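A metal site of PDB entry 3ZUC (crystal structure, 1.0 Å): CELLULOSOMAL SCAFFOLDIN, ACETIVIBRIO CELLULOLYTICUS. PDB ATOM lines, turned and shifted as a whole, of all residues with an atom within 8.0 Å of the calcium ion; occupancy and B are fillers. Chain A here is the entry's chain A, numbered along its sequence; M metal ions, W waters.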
ATOM      1  N   ALA A  17       3.904  -5.836  -1.494  1.00  0.00           N
ATOM      2  CA  ALA A  17       2.864  -6.836  -1.788  1.00  0.00           C
ATOM      3  C   ALA A  17       2.981  -7.334  -3.218  1.00  0.00           C
ATOM      4  O   ALA A  17       3.011  -8.543  -3.475  1.00  0.00           O
ATOM      5  CB  ALA A  17       1.482  -6.298  -1.492  1.00  0.00           C
ATOM      6  N   ILE A  22      10.653 -12.881  -4.092  1.00  0.00           N
ATOM      7  CA  ILE A  22      10.449 -13.124  -2.677  1.00  0.00           C
ATOM      8  C   ILE A  22      11.840 -13.306  -2.065  1.00  0.00           C
ATOM      9  O   ILE A  22      12.739 -13.903  -2.665  1.00  0.00           O
ATOM     10  CB  ILE A  22       9.485 -14.312  -2.458  1.00  0.00           C
ATOM     11  CG1 ILE A  22       8.103 -13.918  -3.037  1.00  0.00           C
ATOM     12  CG2 ILE A  22       9.364 -14.658  -0.990  1.00  0.00           C
ATOM     13  CD1 ILE A  22       7.072 -15.019  -3.051  1.00  0.00           C
ATOM     14  N   TYR A  46       6.185 -21.234   2.583  1.00  0.00           N
ATOM     15  CA  TYR A  46       4.903 -21.522   1.958  1.00  0.00           C
ATOM     16  C   TYR A  46       4.260 -20.264   1.384  1.00  0.00           C
ATOM     17  O   TYR A  46       4.257 -19.198   2.026  1.00  0.00           O
ATOM     18  CB  TYR A  46       3.960 -22.110   3.013  1.00  0.00           C
ATOM     19  CG  TYR A  46       4.417 -23.427   3.594  1.00  0.00           C
ATOM     20  CD1 TYR A  46       4.109 -24.615   2.954  1.00  0.00           C
ATOM     21  CD2 TYR A  46       5.174 -23.490   4.749  1.00  0.00           C
ATOM     22  CE1 TYR A  46       4.522 -25.837   3.425  1.00  0.00           C
ATOM     23  CE2 TYR A  46       5.590 -24.706   5.249  1.00  0.00           C
ATOM     24  CZ  TYR A  46       5.277 -25.882   4.593  1.00  0.00           C
ATOM     25  OH  TYR A  46       5.697 -27.092   5.122  1.00  0.00           O
ATOM     26  N   PHE A  47       3.681 -20.388   0.205  1.00  0.00           N
ATOM     27  CA  PHE A  47       3.150 -19.228  -0.476  1.00  0.00           C
ATOM     28  C   PHE A  47       2.094 -19.646  -1.506  1.00  0.00           C
ATOM     29  O   PHE A  47       1.951 -20.823  -1.837  1.00  0.00           O
ATOM     30  CB  PHE A  47       4.304 -18.433  -1.148  1.00  0.00           C
ATOM     31  CG  PHE A  47       5.051 -19.176  -2.221  1.00  0.00           C
ATOM     32  CD1 PHE A  47       6.045 -20.108  -1.910  1.00  0.00           C
ATOM     33  CD2 PHE A  47       4.792 -18.935  -3.576  1.00  0.00           C
ATOM     34  CE1 PHE A  47       6.740 -20.771  -2.909  1.00  0.00           C
ATOM     35  CE2 PHE A  47       5.484 -19.594  -4.558  1.00  0.00           C
ATOM     36  CZ  PHE A  47       6.464 -20.515  -4.235  1.00  0.00           C
ATOM     37  N   THR A  48       1.384 -18.646  -2.026  1.00  0.00           N
ATOM     38  CA  THR A  48       0.550 -18.817  -3.207  1.00  0.00           C
ATOM     39  C   THR A  48       1.276 -18.185  -4.389  1.00  0.00           C
ATOM     40  O   THR A  48       1.713 -17.032  -4.310  1.00  0.00           O
ATOM     41  CB  THR A  48      -0.855 -18.251  -3.073  1.00  0.00           C
ATOM     42  OG1 THR A  48      -0.757 -16.834  -2.914  1.00  0.00           O
ATOM     43  CG2 THR A  48      -1.592 -18.862  -1.899  1.00  0.00           C
ATOM     44  N   VAL A  49       1.453 -18.950  -5.457  1.00  0.00           N
ATOM     45  CA  VAL A  49       2.311 -18.534  -6.556  1.00  0.00           C
ATOM     46  C   VAL A  49       1.779 -17.375  -7.388  1.00  0.00           C
ATOM     47  O   VAL A  49       2.562 -16.652  -7.991  1.00  0.00           O
ATOM     48  CB  VAL A  49       2.683 -19.769  -7.423  1.00  0.00           C
ATOM     49  CG1 VAL A  49       1.475 -20.297  -8.204  1.00  0.00           C
ATOM     50  CG2 VAL A  49       3.857 -19.517  -8.348  1.00  0.00           C
ATOM     51  N   ASP A  50       0.450 -17.202  -7.443  1.00  0.00           N
ATOM     52  CA  ASP A  50      -0.167 -16.116  -8.210  1.00  0.00           C
ATOM     53  C   ASP A  50       0.268 -16.160  -9.688  1.00  0.00           C
ATOM     54  O   ASP A  50       0.795 -15.195 -10.240  1.00  0.00           O
ATOM     55  CB  ASP A  50       0.150 -14.759  -7.594  1.00  0.00           C
ATOM     56  CG  ASP A  50      -0.425 -14.606  -6.222  1.00  0.00           C
ATOM     57  OD1 ASP A  50      -1.670 -14.716  -6.125  1.00  0.00           O
ATOM     58  OD2 ASP A  50       0.320 -14.366  -5.267  1.00  0.00           O
ATOM     59  N   GLY A  51       0.008 -17.318 -10.309  1.00  0.00           N
ATOM     60  CA  GLY A  51       0.411 -17.574 -11.673  1.00  0.00           C
ATOM     61  C   GLY A  51       1.650 -18.461 -11.676  1.00  0.00           C
ATOM     62  O   GLY A  51       2.758 -18.002 -11.456  1.00  0.00           O
ATOM     63  N   GLY A  82      -3.353 -19.678   1.959  1.00  0.00           N
ATOM     64  CA  GLY A  82      -2.035 -19.097   1.931  1.00  0.00           C
ATOM     65  C   GLY A  82      -0.944 -19.960   1.347  1.00  0.00           C
ATOM     66  O   GLY A  82       0.218 -19.526   1.328  1.00  0.00           O
ATOM     67  N   ALA A  83      -1.269 -21.159   0.870  1.00  0.00           N
ATOM     68  CA  ALA A  83      -0.225 -22.081   0.449  1.00  0.00           C
ATOM     69  C   ALA A  83      -0.690 -22.987  -0.675  1.00  0.00           C
ATOM     70  O   ALA A  83      -1.412 -23.966  -0.450  1.00  0.00           O
ATOM     71  CB  ALA A  83       0.239 -22.922   1.642  1.00  0.00           C
ATOM     72  N   ASP A  84      -0.253 -22.686  -1.896  1.00  0.00           N
ATOM     73  CA  ASP A  84      -0.369 -23.621  -3.002  1.00  0.00           C
ATOM     74  C   ASP A  84       0.983 -24.201  -3.419  1.00  0.00           C
ATOM     75  O   ASP A  84       0.988 -25.169  -4.170  1.00  0.00           O
ATOM     76  CB  ASP A  84      -1.209 -23.105  -4.177  1.00  0.00           C
ATOM     77  CG  ASP A  84      -0.690 -21.853  -4.815  1.00  0.00           C
ATOM     78  OD1 ASP A  84       0.528 -21.616  -4.852  1.00  0.00           O
ATOM     79  OD2 ASP A  84      -1.554 -21.055  -5.250  1.00  0.00           O
ATOM     80  N   LYS A 112      10.174 -15.938 -10.713  1.00  0.00           N
ATOM     81  CA  LYS A 112       9.646 -16.688 -11.846  1.00  0.00           C
ATOM     82  C   LYS A 112      10.517 -16.473 -13.078  1.00  0.00           C
ATOM     83  O   LYS A 112      11.191 -15.452 -13.233  1.00  0.00           O
ATOM     84  CB  LYS A 112       8.229 -16.203 -12.146  1.00  0.00           C
ATOM     85  CG  LYS A 112       7.286 -16.400 -10.979  1.00  0.00           C
ATOM     86  CD  LYS A 112       5.885 -15.867 -11.288  1.00  0.00           C
ATOM     87  CE  LYS A 112       5.051 -15.894 -10.049  1.00  0.00           C
ATOM     88  NZ  LYS A 112       3.643 -15.492 -10.296  1.00  0.00           N
ATOM     89  N   ASN A 117       4.920 -11.003 -11.550  1.00  0.00           N
ATOM     90  CA  ASN A 117       4.734 -10.709 -10.141  1.00  0.00           C
ATOM     91  C   ASN A 117       4.095 -11.805  -9.316  1.00  0.00           C
ATOM     92  O   ASN A 117       3.267 -12.601  -9.788  1.00  0.00           O
ATOM     93  CB  ASN A 117       3.911  -9.439  -9.964  1.00  0.00           C
ATOM     94  CG  ASN A 117       4.676  -8.188 -10.378  1.00  0.00           C
ATOM     95  OD1 ASN A 117       5.900  -8.142 -10.324  1.00  0.00           O
ATOM     96  ND2 ASN A 117       3.939  -7.175 -10.791  1.00  0.00           N
ATOM     97  N   TYR A 118       4.464 -11.789  -8.042  1.00  0.00           N
ATOM     98  CA  TYR A 118       3.790 -12.422  -6.942  1.00  0.00           C
ATOM     99  C   TYR A 118       2.911 -11.399  -6.199  1.00  0.00           C
ATOM    100  O   TYR A 118       3.195 -10.201  -6.254  1.00  0.00           O
ATOM    101  CB  TYR A 118       4.809 -12.922  -5.915  1.00  0.00           C
ATOM    102  CG  TYR A 118       5.765 -13.977  -6.401  1.00  0.00           C
ATOM    103  CD1 TYR A 118       5.405 -15.316  -6.408  1.00  0.00           C
ATOM    104  CD2 TYR A 118       7.037 -13.661  -6.818  1.00  0.00           C
ATOM    105  CE1 TYR A 118       6.292 -16.307  -6.802  1.00  0.00           C
ATOM    106  CE2 TYR A 118       7.925 -14.625  -7.218  1.00  0.00           C
ATOM    107  CZ  TYR A 118       7.569 -15.957  -7.196  1.00  0.00           C
ATOM    108  OH  TYR A 118       8.476 -16.891  -7.618  1.00  0.00           O
ATOM    109  N   ASN A 119       1.894 -11.878  -5.474  1.00  0.00           N
ATOM    110  CA  ASN A 119       1.242 -11.119  -4.395  1.00  0.00           C
ATOM    111  C   ASN A 119       1.700 -11.710  -3.074  1.00  0.00           C
ATOM    112  O   ASN A 119       1.265 -12.796  -2.687  1.00  0.00           O
ATOM    113  CB  ASN A 119      -0.283 -11.196  -4.488  1.00  0.00           C
ATOM    114  CG  ASN A 119      -0.951 -10.601  -3.280  1.00  0.00           C
ATOM    115  OD1 ASN A 119      -0.396  -9.708  -2.638  1.00  0.00           O
ATOM    116  ND2 ASN A 119      -2.138 -11.090  -2.950  1.00  0.00           N
ATOM    117  N   GLN A 120       2.605 -11.035  -2.383  1.00  0.00           N
ATOM    118  CA  GLN A 120       3.127 -11.576  -1.135  1.00  0.00           C
ATOM    119  C   GLN A 120       2.096 -11.582  -0.020  1.00  0.00           C
ATOM    120  O   GLN A 120       2.211 -12.359   0.939  1.00  0.00           O
ATOM    121  CB  GLN A 120       4.370 -10.813  -0.668  1.00  0.00           C
ATOM    122  CG  GLN A 120       5.489 -10.786  -1.671  1.00  0.00           C
ATOM    123  CD  GLN A 120       6.820 -10.579  -1.005  1.00  0.00           C
ATOM    124  OE1 GLN A 120       7.384 -11.532  -0.456  1.00  0.00           O
ATOM    125  NE2 GLN A 120       7.323  -9.348  -1.007  1.00  0.00           N
ATOM    126  N   ALA A 121       1.112 -10.689  -0.095  1.00  0.00           N
ATOM    127  CA  ALA A 121       0.277 -10.399   1.065  1.00  0.00           C
ATOM    128  C   ALA A 121      -0.506 -11.606   1.567  1.00  0.00           C
ATOM    129  O   ALA A 121      -0.791 -11.691   2.765  1.00  0.00           O
ATOM    130  CB  ALA A 121      -0.687  -9.263   0.762  1.00  0.00           C
ATOM    131  N   ASP A 122      -0.873 -12.518   0.660  1.00  0.00           N
ATOM    132  CA  ASP A 122      -1.639 -13.703   1.045  1.00  0.00           C
ATOM    133  C   ASP A 122      -0.792 -14.921   1.366  1.00  0.00           C
ATOM    134  O   ASP A 122      -1.352 -15.986   1.618  1.00  0.00           O
ATOM    135  CB  ASP A 122      -2.674 -14.050  -0.018  1.00  0.00           C
ATOM    136  CG  ASP A 122      -2.076 -14.612  -1.294  1.00  0.00           C
ATOM    137  OD1 ASP A 122      -0.915 -14.273  -1.620  1.00  0.00           O
ATOM    138  OD2 ASP A 122      -2.788 -15.382  -1.989  1.00  0.00           O
ATOM    139  N   ASP A 123       0.525 -14.805   1.377  1.00  0.00           N
ATOM    140  CA  ASP A 123       1.351 -15.986   1.540  1.00  0.00           C
ATOM    141  C   ASP A 123       1.442 -16.417   2.993  1.00  0.00           C
ATOM    142  O   ASP A 123       1.724 -15.599   3.873  1.00  0.00           O
ATOM    143  CB  ASP A 123       2.764 -15.702   1.005  1.00  0.00           C
ATOM    144  CG  ASP A 123       2.792 -15.481  -0.495  1.00  0.00           C
ATOM    145  OD1 ASP A 123       1.835 -15.917  -1.178  1.00  0.00           O
ATOM    146  OD2 ASP A 123       3.810 -14.915  -0.982  1.00  0.00           O
ATOM    147  N   TYR A 124       1.275 -17.701   3.241  1.00  0.00           N
ATOM    148  CA  TYR A 124       1.284 -18.260   4.591  1.00  0.00           C
ATOM    149  C   TYR A 124       2.535 -17.845   5.366  1.00  0.00           C
ATOM    150  O   TYR A 124       2.434 -17.482   6.543  1.00  0.00           O
ATOM    151  CB  TYR A 124       1.195 -19.792   4.498  1.00  0.00           C
ATOM    152  CG  TYR A 124       1.219 -20.542   5.785  1.00  0.00           C
ATOM    153  CD1 TYR A 124       2.400 -20.994   6.362  1.00  0.00           C
ATOM    154  CD2 TYR A 124       0.034 -20.888   6.405  1.00  0.00           C
ATOM    155  CE1 TYR A 124       2.400 -21.736   7.522  1.00  0.00           C
ATOM    156  CE2 TYR A 124       0.014 -21.621   7.565  1.00  0.00           C
ATOM    157  CZ  TYR A 124       1.194 -22.040   8.128  1.00  0.00           C
ATOM    158  OH  TYR A 124       1.153 -22.778   9.292  1.00  0.00           O
ATOM    159  N   PHE A 126       4.699 -15.290   4.712  1.00  0.00           N
ATOM    160  CA  PHE A 126       5.159 -13.905   4.580  1.00  0.00           C
ATOM    161  C   PHE A 126       4.940 -13.121   5.865  1.00  0.00           C
ATOM    162  O   PHE A 126       3.867 -13.174   6.466  1.00  0.00           O
ATOM    163  CB  PHE A 126       4.361 -13.240   3.459  1.00  0.00           C
ATOM    164  CG  PHE A 126       4.707 -11.779   3.215  1.00  0.00           C
ATOM    165  CD1 PHE A 126       5.962 -11.399   2.786  1.00  0.00           C
ATOM    166  CD2 PHE A 126       3.722 -10.804   3.324  1.00  0.00           C
ATOM    167  CE1 PHE A 126       6.265 -10.082   2.505  1.00  0.00           C
ATOM    168  CE2 PHE A 126       4.007  -9.483   3.027  1.00  0.00           C
ATOM    169  CZ  PHE A 126       5.279  -9.121   2.617  1.00  0.00           C
HETATM  170 CA    CA M   1       0.815 -15.052  -3.112  1.00  0.00          CA
HETATM  171  O   HOH W   1       3.216 -14.758  -3.606  1.00  0.00           O
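The calcium ion is bound by the side-chain carboxylate (OD2) of Asp 50 (2.3 Å), the backbone carbonyl oxygen (O) of Asn 119 (2.3 Å), the side-chain carboxylate (OD1) of Asp 123 (2.4 Å), the side-chain hydroxyl (OG1) of Thr 48 (2.4 Å), the side-chain carboxylate (OD1) of Asp 122 (2.4 Å), water W1 (2.5 Å) and the backbone carbonyl oxygen (O) of Thr 48 (2.5 Å).
The calcium ion has seven donor atoms within binding distance.
N of Ala 121 lies within hydrogen-bond range of OD1 of Asn 119 (3.1 Å).
The side-chain amino group of Lys 112 sits at hydrogen-bond distance from the backbone carbonyl oxygen of Asp 50 (2.9 Å).
The nearest printed residue that does not touch the calcium ion is Gln 120 (4.5 Å).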
